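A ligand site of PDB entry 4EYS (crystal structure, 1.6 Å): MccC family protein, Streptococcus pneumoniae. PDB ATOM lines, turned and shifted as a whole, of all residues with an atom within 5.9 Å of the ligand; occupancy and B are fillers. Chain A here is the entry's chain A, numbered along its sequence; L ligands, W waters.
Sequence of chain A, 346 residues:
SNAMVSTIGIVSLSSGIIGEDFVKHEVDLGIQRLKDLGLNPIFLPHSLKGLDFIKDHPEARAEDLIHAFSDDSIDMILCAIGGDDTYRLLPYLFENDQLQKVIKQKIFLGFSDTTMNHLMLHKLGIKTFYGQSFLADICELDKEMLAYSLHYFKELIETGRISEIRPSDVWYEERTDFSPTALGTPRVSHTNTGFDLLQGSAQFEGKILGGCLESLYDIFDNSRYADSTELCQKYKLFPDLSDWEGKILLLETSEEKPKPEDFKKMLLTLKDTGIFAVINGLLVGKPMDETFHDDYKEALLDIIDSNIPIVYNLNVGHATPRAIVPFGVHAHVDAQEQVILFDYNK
Residues that only touch the ligand: Ile 81 (3.5 Å), Gly 83 (3.97 Å), Phe 111 (3.7 Å), Leu 135 (3.4 Å), Ala 136 (3.5 Å) and Phe 178 (3.2 Å).
Within 4 Å of the ligand: Glu 26, Ile 81, Gly 82, Gly 83, Phe 111, Ser 112, Leu 135, Ala 136, Glu 174, Phe 178, Glu 255, Met 288, His 318 and Arg 322.
The nearest printed residue that does not touch the ligand is Val 23 (4.1 Å).
OE1 of Glu 174 is in salt-bridge range of NH1 of Arg 187, at 2.7 Å.
O of Glu 26 is in hydrogen-bond range of SG of Cys 139, 3.1 Å away.
OE2 of Glu 255 sits close to NE2 of His 318, at 3.4 Å.
A ring nitrogen (NE2) of His 318 sits at hydrogen-bond distance from the side-chain hydroxyl (OG) of Ser 112, at 2.9 Å.
The backbone carbonyl oxygen (O) of His 318 lies within hydrogen-bond range of the guanidinium group (NH1) of Arg 322 (3.0 Å).
NH2 of Arg 322 lies within hydrogen-bond range of O of Ala 136, at 3.4 Å.
The guanidinium group (NE) of Arg 322 sits at hydrogen-bond distance from the backbone carbonyl oxygen (O) of Ala 319 (3.3 Å).
The backbone NH of Ala 136 sits close to the side-chain hydroxyl of Ser 133 (3.5 Å).
The side-chain carboxylate (OE2) of Glu 174 sits at hydrogen-bond distance from an oxygen (O7) of the ligand (2.6 Å).
A nitrogen (N4) of the ligand lies within hydrogen-bond range of the side-chain carboxylate (OE1) of Glu 26 (2.6 Å).
O1 of the ligand lies close to OE2 of Glu 255 (2.7 Å).
O3 of the ligand sits at hydrogen-bond distance from N of Gly 82, 2.8 Å away.
O of His 318 sits at hydrogen-bond distance from O6 of the ligand (3.5 Å).
A ring nitrogen (NE2) of His 318 lies within hydrogen-bond range of an oxygen (O1) of the ligand (2.8 Å).
OG of Ser 112 sits at hydrogen-bond distance from O1 of the ligand, at 2.9 Å.
An oxygen (O6) of the ligand is in hydrogen-bond range of the guanidinium group (NH1) of Arg 322 (3.2 Å).
The side-chain sulfur (SD) of Met 288 sits at hydrogen-bond distance from an oxygen (O6) of the ligand (3.5 Å).
Water W7 lies within hydrogen-bond range of an oxygen (O2) of the ligand, the side-chain carboxylate (OE1) of Glu 255 and the backbone carbonyl oxygen (O) of Gly 83.
Water W1 lies within hydrogen-bond range of an oxygen (O3) of the ligand (2.8 Å), the side-chain hydroxyl of Ser 133 (2.9 Å) and the backbone NH of Gly 82 (3.3 Å).
Water W8 bridges an oxygen (O2) of the ligand (2.8 Å) and the backbone carbonyl oxygen of Gly 82 (3.1 Å).
Water W5 lies within hydrogen-bond range of the backbone carbonyl oxygen of Ala 136 (2.9 Å), the guanidinium group of Arg 187 (2.9 Å) and a nitrogen (N5) of the ligand (3.5 Å).
Water W6 lies within hydrogen-bond range of the side-chain hydroxyl (OG) of Ser 112 (2.5 Å), the backbone carbonyl oxygen (O) of Gly 83 (2.7 Å), the backbone NH (N) of Asp 113 (3.1 Å) and an oxygen (O1) of the ligand (3.3 Å).
Water W4 bridges the side-chain carboxylate (OE1) of Glu 26 (2.7 Å) and the backbone carbonyl oxygen (O) of Cys 139 (2.7 Å).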
ATOM      1  N   ILE A  17     -14.762  16.099   5.779  1.00  0.00           N
ATOM      2  CA  ILE A  17     -15.963  16.626   6.473  1.00  0.00           C
ATOM      3  C   ILE A  17     -16.310  15.881   7.821  1.00  0.00           C
ATOM      4  O   ILE A  17     -16.825  16.561   8.691  1.00  0.00           O
ATOM      5  CB  ILE A  17     -17.186  16.648   5.566  1.00  0.00           C
ATOM      6  CG1 ILE A  17     -18.356  17.478   6.191  1.00  0.00           C
ATOM      7  CG2 ILE A  17     -17.625  15.253   5.166  1.00  0.00           C
ATOM      8  CD1 ILE A  17     -19.490  17.644   5.235  1.00  0.00           C
ATOM      9  N   PHE A  22     -20.033  20.614  12.728  1.00  0.00           N
ATOM     10  CA  PHE A  22     -21.378  20.787  12.185  1.00  0.00           C
ATOM     11  C   PHE A  22     -22.082  19.499  11.657  1.00  0.00           C
ATOM     12  O   PHE A  22     -23.265  19.567  11.322  1.00  0.00           O
ATOM     13  CB  PHE A  22     -21.467  21.912  11.168  1.00  0.00           C
ATOM     14  CG  PHE A  22     -20.797  21.636   9.840  1.00  0.00           C
ATOM     15  CD1 PHE A  22     -19.457  21.962   9.635  1.00  0.00           C
ATOM     16  CD2 PHE A  22     -21.526  21.141   8.787  1.00  0.00           C
ATOM     17  CE1 PHE A  22     -18.869  21.723   8.410  1.00  0.00           C
ATOM     18  CE2 PHE A  22     -20.931  20.873   7.542  1.00  0.00           C
ATOM     19  CZ  PHE A  22     -19.601  21.151   7.369  1.00  0.00           C
ATOM     20  N   VAL A  23     -21.308  18.402  11.507  1.00  0.00           N
ATOM     21  CA  VAL A  23     -21.861  17.086  11.196  1.00  0.00           C
ATOM     22  C   VAL A  23     -21.802  16.089  12.354  1.00  0.00           C
ATOM     23  O   VAL A  23     -22.164  14.932  12.180  1.00  0.00           O
ATOM     24  CB  VAL A  23     -21.223  16.459   9.926  1.00  0.00           C
ATOM     25  CG1 VAL A  23     -21.428  17.485   8.791  1.00  0.00           C
ATOM     26  CG2 VAL A  23     -19.793  16.106  10.196  1.00  0.00           C
ATOM     27  N   GLU A  26     -24.656  13.860  13.029  1.00  0.00           N
ATOM     28  CA  GLU A  26     -24.833  12.803  12.049  1.00  0.00           C
ATOM     29  C   GLU A  26     -23.877  11.645  12.300  1.00  0.00           C
ATOM     30  O   GLU A  26     -24.240  10.482  12.226  1.00  0.00           O
ATOM     31  CB  GLU A  26     -24.639  13.349  10.587  1.00  0.00           C
ATOM     32  CG  GLU A  26     -25.371  14.616  10.247  1.00  0.00           C
ATOM     33  CD  GLU A  26     -25.210  14.946   8.756  1.00  0.00           C
ATOM     34  OE1 GLU A  26     -25.738  14.186   7.930  1.00  0.00           O
ATOM     35  OE2 GLU A  26     -24.592  15.999   8.478  1.00  0.00           O
ATOM     36  N   ILE A  81     -17.110   9.366   2.921  1.00  0.00           N
ATOM     37  CA  ILE A  81     -17.792  10.257   2.008  1.00  0.00           C
ATOM     38  C   ILE A  81     -16.815  10.518   0.808  1.00  0.00           C
ATOM     39  O   ILE A  81     -15.657  10.188   0.916  1.00  0.00           O
ATOM     40  CB  ILE A  81     -18.197  11.659   2.690  1.00  0.00           C
ATOM     41  CG1 ILE A  81     -19.206  12.412   1.830  1.00  0.00           C
ATOM     42  CG2 ILE A  81     -16.903  12.442   3.031  1.00  0.00           C
ATOM     43  CD1 ILE A  81     -20.602  11.833   1.691  1.00  0.00           C
ATOM     44  N   GLY A  82     -17.351  11.025  -0.286  1.00  0.00           N
ATOM     45  CA  GLY A  82     -16.557  11.379  -1.480  1.00  0.00           C
ATOM     46  C   GLY A  82     -16.016  12.793  -1.359  1.00  0.00           C
ATOM     47  O   GLY A  82     -15.672  13.259  -0.270  1.00  0.00           O
ATOM     48  N   GLY A  83     -15.871  13.414  -2.518  1.00  0.00           N
ATOM     49  CA  GLY A  83     -15.122  14.628  -2.619  1.00  0.00           C
ATOM     50  C   GLY A  83     -14.678  14.727  -4.043  1.00  0.00           C
ATOM     51  O   GLY A  83     -15.395  14.344  -4.904  1.00  0.00           O
ATOM     52  N   PHE A 111     -18.489   5.314  -2.670  1.00  0.00           N
ATOM     53  CA  PHE A 111     -18.899   5.760  -3.985  1.00  0.00           C
ATOM     54  C   PHE A 111     -18.425   7.184  -4.287  1.00  0.00           C
ATOM     55  O   PHE A 111     -17.730   7.751  -3.526  1.00  0.00           O
ATOM     56  CB  PHE A 111     -20.402   5.569  -4.250  1.00  0.00           C
ATOM     57  CG  PHE A 111     -21.340   6.494  -3.520  1.00  0.00           C
ATOM     58  CD1 PHE A 111     -21.538   6.341  -2.153  1.00  0.00           C
ATOM     59  CD2 PHE A 111     -22.089   7.450  -4.213  1.00  0.00           C
ATOM     60  CE1 PHE A 111     -22.454   7.150  -1.526  1.00  0.00           C
ATOM     61  CE2 PHE A 111     -22.984   8.303  -3.538  1.00  0.00           C
ATOM     62  CZ  PHE A 111     -23.202   8.076  -2.175  1.00  0.00           C
ATOM     63  N   SER A 112     -18.804   7.654  -5.471  1.00  0.00           N
ATOM     64  CA  SER A 112     -18.520   9.048  -5.876  1.00  0.00           C
ATOM     65  C   SER A 112     -17.014   9.215  -6.204  1.00  0.00           C
ATOM     66  O   SER A 112     -16.501   8.414  -7.014  1.00  0.00           O
ATOM     67  CB  SER A 112     -19.070  10.038  -4.875  1.00  0.00           C
ATOM     68  OG  SER A 112     -19.281  11.233  -5.712  1.00  0.00           O
ATOM     69  N   ASP A 113     -16.260  10.114  -5.561  1.00  0.00           N
ATOM     70  CA  ASP A 113     -14.794  10.253  -5.819  1.00  0.00           C
ATOM     71  C   ASP A 113     -14.111   8.904  -5.559  1.00  0.00           C
ATOM     72  O   ASP A 113     -13.047   8.640  -6.032  1.00  0.00           O
ATOM     73  CB  ASP A 113     -14.218  11.352  -4.899  1.00  0.00           C
ATOM     74  CG  ASP A 113     -12.736  11.673  -5.145  1.00  0.00           C
ATOM     75  OD1 ASP A 113     -12.393  11.863  -6.346  1.00  0.00           O
ATOM     76  OD2 ASP A 113     -11.993  11.825  -4.187  1.00  0.00           O
ATOM     77  N   SER A 133     -21.795   5.015   1.486  1.00  0.00           N
ATOM     78  CA  SER A 133     -20.757   5.520   2.363  1.00  0.00           C
ATOM     79  C   SER A 133     -21.266   5.749   3.759  1.00  0.00           C
ATOM     80  O   SER A 133     -22.452   5.727   3.963  1.00  0.00           O
ATOM     81  CB  SER A 133     -20.109   6.782   1.763  1.00  0.00           C
ATOM     82  OG  SER A 133     -21.026   7.868   1.738  1.00  0.00           O
ATOM     83  N   LEU A 135     -21.210   8.599   5.812  1.00  0.00           N
ATOM     84  CA  LEU A 135     -22.015   9.809   5.962  1.00  0.00           C
ATOM     85  C   LEU A 135     -23.307   9.787   5.185  1.00  0.00           C
ATOM     86  O   LEU A 135     -24.325  10.231   5.651  1.00  0.00           O
ATOM     87  CB  LEU A 135     -21.169  11.084   5.744  1.00  0.00           C
ATOM     88  CG  LEU A 135     -21.868  12.425   5.996  1.00  0.00           C
ATOM     89  CD1 LEU A 135     -22.411  12.515   7.418  1.00  0.00           C
ATOM     90  CD2 LEU A 135     -20.909  13.606   5.709  1.00  0.00           C
ATOM     91  N   ALA A 136     -23.247   9.316   3.961  1.00  0.00           N
ATOM     92  CA  ALA A 136     -24.378   9.352   3.064  1.00  0.00           C
ATOM     93  C   ALA A 136     -25.522   8.374   3.425  1.00  0.00           C
ATOM     94  O   ALA A 136     -26.702   8.692   3.225  1.00  0.00           O
ATOM     95  CB  ALA A 136     -23.934   9.136   1.608  1.00  0.00           C
ATOM     96  N   CYS A 139     -25.440   7.223   8.190  1.00  0.00           N
ATOM     97  CA  CYS A 139     -25.817   8.384   9.032  1.00  0.00           C
ATOM     98  C   CYS A 139     -27.184   8.995   8.649  1.00  0.00           C
ATOM     99  O   CYS A 139     -27.499  10.150   8.964  1.00  0.00           O
ATOM    100  CB  CYS A 139     -24.679   9.414   9.074  1.00  0.00           C
ATOM    101  SG  CYS A 139     -23.169   8.914   9.761  1.00  0.00           S
ATOM    102  N   LEU A 141     -30.580  10.473   8.539  1.00  0.00           N
ATOM    103  CA  LEU A 141     -31.109  11.299   9.658  1.00  0.00           C
ATOM    104  C   LEU A 141     -32.501  10.936  10.091  1.00  0.00           C
ATOM    105  O   LEU A 141     -32.936  11.434  11.058  1.00  0.00           O
ATOM    106  CB  LEU A 141     -31.083  12.818   9.347  1.00  0.00           C
ATOM    107  CG  LEU A 141     -29.715  13.473   9.275  1.00  0.00           C
ATOM    108  CD1 LEU A 141     -29.894  14.844   8.624  1.00  0.00           C
ATOM    109  CD2 LEU A 141     -28.995  13.607  10.619  1.00  0.00           C
ATOM    110  N   GLU A 174     -32.915  14.268  -2.290  1.00  0.00           N
ATOM    111  CA  GLU A 174     -31.898  14.659  -1.331  1.00  0.00           C
ATOM    112  C   GLU A 174     -32.401  15.740  -0.386  1.00  0.00           C
ATOM    113  O   GLU A 174     -33.168  16.635  -0.781  1.00  0.00           O
ATOM    114  CB  GLU A 174     -30.595  15.098  -2.008  1.00  0.00           C
ATOM    115  CG  GLU A 174     -29.438  15.330  -1.057  1.00  0.00           C
ATOM    116  CD  GLU A 174     -29.056  14.138  -0.184  1.00  0.00           C
ATOM    117  OE1 GLU A 174     -29.831  13.753   0.751  1.00  0.00           O
ATOM    118  OE2 GLU A 174     -27.937  13.622  -0.389  1.00  0.00           O
ATOM    119  N   PHE A 178     -29.608  19.159   6.748  1.00  0.00           N
ATOM    120  CA  PHE A 178     -28.853  18.058   7.453  1.00  0.00           C
ATOM    121  C   PHE A 178     -28.486  18.410   8.889  1.00  0.00           C
ATOM    122  O   PHE A 178     -27.747  17.692   9.583  1.00  0.00           O
ATOM    123  CB  PHE A 178     -27.557  17.680   6.705  1.00  0.00           C
ATOM    124  CG  PHE A 178     -27.784  17.014   5.379  1.00  0.00           C
ATOM    125  CD1 PHE A 178     -27.990  15.645   5.287  1.00  0.00           C
ATOM    126  CD2 PHE A 178     -27.720  17.746   4.179  1.00  0.00           C
ATOM    127  CE1 PHE A 178     -28.136  15.019   4.056  1.00  0.00           C
ATOM    128  CE2 PHE A 178     -27.890  17.115   2.953  1.00  0.00           C
ATOM    129  CZ  PHE A 178     -28.115  15.754   2.882  1.00  0.00           C
ATOM    130  N   ARG A 187     -37.481  11.943   4.318  1.00  0.00           N
ATOM    131  CA  ARG A 187     -37.207  12.424   2.993  1.00  0.00           C
ATOM    132  C   ARG A 187     -38.462  12.455   2.202  1.00  0.00           C
ATOM    133  O   ARG A 187     -39.427  11.754   2.456  1.00  0.00           O
ATOM    134  CB  ARG A 187     -36.179  11.496   2.292  1.00  0.00           C
ATOM    135  CG  ARG A 187     -34.764  11.658   2.805  1.00  0.00           C
ATOM    136  CD  ARG A 187     -33.907  10.544   2.215  1.00  0.00           C
ATOM    137  NE  ARG A 187     -32.536  10.511   2.689  1.00  0.00           N
ATOM    138  CZ  ARG A 187     -31.543  11.169   2.137  1.00  0.00           C
ATOM    139  NH1 ARG A 187     -31.762  11.915   1.077  1.00  0.00           N
ATOM    140  NH2 ARG A 187     -30.316  11.018   2.638  1.00  0.00           N
ATOM    141  N   SER A 254     -23.263  12.749 -10.057  1.00  0.00           N
ATOM    142  CA  SER A 254     -23.094  13.238  -8.717  1.00  0.00           C
ATOM    143  C   SER A 254     -24.090  14.428  -8.427  1.00  0.00           C
ATOM    144  O   SER A 254     -24.892  14.827  -9.246  1.00  0.00           O
ATOM    145  CB  SER A 254     -21.676  13.701  -8.450  1.00  0.00           C
ATOM    146  OG  SER A 254     -21.418  14.946  -9.027  1.00  0.00           O
ATOM    147  N   GLU A 255     -23.903  14.975  -7.224  1.00  0.00           N
ATOM    148  CA  GLU A 255     -24.634  16.162  -6.761  1.00  0.00           C
ATOM    149  C   GLU A 255     -24.304  17.401  -7.603  1.00  0.00           C
ATOM    150  O   GLU A 255     -25.025  18.430  -7.566  1.00  0.00           O
ATOM    151  CB  GLU A 255     -24.361  16.416  -5.275  1.00  0.00           C
ATOM    152  CG  GLU A 255     -23.008  16.960  -4.879  1.00  0.00           C
ATOM    153  CD  GLU A 255     -21.883  15.939  -4.896  1.00  0.00           C
ATOM    154  OE1 GLU A 255     -20.702  16.422  -4.934  1.00  0.00           O
ATOM    155  OE2 GLU A 255     -22.143  14.702  -4.905  1.00  0.00           O
ATOM    156  N   MET A 288     -29.259  12.161  -9.334  1.00  0.00           N
ATOM    157  CA  MET A 288     -29.697  12.728  -8.054  1.00  0.00           C
ATOM    158  C   MET A 288     -30.889  13.643  -8.269  1.00  0.00           C
ATOM    159  O   MET A 288     -30.956  14.490  -9.149  1.00  0.00           O
ATOM    160  CB  MET A 288     -28.557  13.461  -7.380  1.00  0.00           C
ATOM    161  CG  MET A 288     -28.873  13.760  -5.895  1.00  0.00           C
ATOM    162  SD  MET A 288     -27.430  14.437  -4.875  1.00  0.00           S
ATOM    163  CE  MET A 288     -28.001  16.220  -4.682  1.00  0.00           C
ATOM    164  N   HIS A 318     -26.074   8.535  -6.678  1.00  0.00           N
ATOM    165  CA  HIS A 318     -26.345   9.723  -5.851  1.00  0.00           C
ATOM    166  C   HIS A 318     -27.801   9.918  -5.424  1.00  0.00           C
ATOM    167  O   HIS A 318     -28.051  10.662  -4.424  1.00  0.00           O
ATOM    168  CB  HIS A 318     -25.704  10.963  -6.427  1.00  0.00           C
ATOM    169  CG  HIS A 318     -24.223  11.004  -6.241  1.00  0.00           C
ATOM    170  ND1 HIS A 318     -23.351  10.196  -6.987  1.00  0.00           N
ATOM    171  CD2 HIS A 318     -23.451  11.730  -5.366  1.00  0.00           C
ATOM    172  CE1 HIS A 318     -22.085  10.521  -6.595  1.00  0.00           C
ATOM    173  NE2 HIS A 318     -22.150  11.421  -5.611  1.00  0.00           N
ATOM    174  N   ALA A 319     -28.753   9.341  -6.165  1.00  0.00           N
ATOM    175  CA  ALA A 319     -30.145   9.371  -5.734  1.00  0.00           C
ATOM    176  C   ALA A 319     -30.209   8.407  -4.542  1.00  0.00           C
ATOM    177  O   ALA A 319     -29.289   7.663  -4.275  1.00  0.00           O
ATOM    178  CB  ALA A 319     -31.079   8.936  -6.820  1.00  0.00           C
ATOM    179  N   ARG A 322     -30.127   3.420  -1.955  1.00  0.00           N
ATOM    180  CA  ARG A 322     -28.872   2.981  -2.648  1.00  0.00           C
ATOM    181  C   ARG A 322     -28.562   1.520  -2.544  1.00  0.00           C
ATOM    182  O   ARG A 322     -28.470   1.005  -1.408  1.00  0.00           O
ATOM    183  CB  ARG A 322     -27.671   3.736  -2.080  1.00  0.00           C
ATOM    184  CG  ARG A 322     -27.744   5.234  -2.309  1.00  0.00           C
ATOM    185  CD  ARG A 322     -26.437   5.935  -2.013  1.00  0.00           C
ATOM    186  NE  ARG A 322     -26.622   7.344  -2.329  1.00  0.00           N
ATOM    187  CZ  ARG A 322     -26.897   8.301  -1.458  1.00  0.00           C
ATOM    188  NH1 ARG A 322     -27.017   9.538  -1.865  1.00  0.00           N
ATOM    189  NH2 ARG A 322     -26.962   8.087  -0.123  1.00  0.00           N
HETATM  190  P1  LIG L   1     -20.365  12.785  -2.147  1.00  0.00           P
HETATM  191  O1  LIG L   1     -20.656  12.818  -3.667  1.00  0.00           O
HETATM  192  O2  LIG L   1     -19.694  14.090  -1.712  1.00  0.00           O
HETATM  193  O3  LIG L   1     -19.623  11.554  -1.762  1.00  0.00           O
HETATM  194  O4  LIG L   1     -21.789  12.798  -1.446  1.00  0.00           O
HETATM  195  C1  LIG L   1     -22.560  11.621  -1.585  1.00  0.00           C
HETATM  196  C2  LIG L   1     -23.935  11.905  -1.053  1.00  0.00           C
HETATM  197  O5  LIG L   1     -23.835  12.406   0.293  1.00  0.00           O
HETATM  198  C3  LIG L   1     -24.651  12.985  -1.912  1.00  0.00           C
HETATM  199  O6  LIG L   1     -25.925  12.511  -2.402  1.00  0.00           O
HETATM  200  C4  LIG L   1     -24.697  14.121  -0.933  1.00  0.00           C
HETATM  201  O7  LIG L   1     -25.831  14.958  -1.102  1.00  0.00           O
HETATM  202  C5  LIG L   1     -24.754  13.464   0.436  1.00  0.00           C
HETATM  203  N1  LIG L   1     -24.333  14.357   1.501  1.00  0.00           N
HETATM  204  C6  LIG L   1     -23.585  15.441   1.437  1.00  0.00           C
HETATM  205  N2  LIG L   1     -23.383  16.006   2.673  1.00  0.00           N
HETATM  206  C7  LIG L   1     -24.066  15.220   3.528  1.00  0.00           C
HETATM  207  C8  LIG L   1     -24.339  15.239   4.955  1.00  0.00           C
HETATM  208  N3  LIG L   1     -23.838  16.172   5.738  1.00  0.00           N
HETATM  209  N4  LIG L   1     -25.052  14.189   5.415  1.00  0.00           N
HETATM  210  C9  LIG L   1     -25.540  13.208   4.674  1.00  0.00           C
HETATM  211  N5  LIG L   1     -25.373  13.184   3.353  1.00  0.00           N
HETATM  212  C10 LIG L   1     -24.642  14.133   2.763  1.00  0.00           C
HETATM  213  O   HOH W   1     -19.969   8.997  -0.746  1.00  0.00           O
HETATM  214  O   HOH W   2     -21.199  17.628   2.196  1.00  0.00           O
HETATM  215  O   HOH W   3     -21.451  16.105  -0.838  1.00  0.00           O
HETATM  216  O   HOH W   4     -27.450  12.247   7.242  1.00  0.00           O
HETATM  217  O   HOH W   5     -27.928  11.026   4.329  1.00  0.00           O
HETATM  218  O   HOH W   6     -17.559  12.743  -4.689  1.00  0.00           O
HETATM  219  O   HOH W   7     -18.466  15.218  -3.769  1.00  0.00           O
HETATM  220  O   HOH W   8     -17.794  15.469  -0.181  1.00  0.00           O
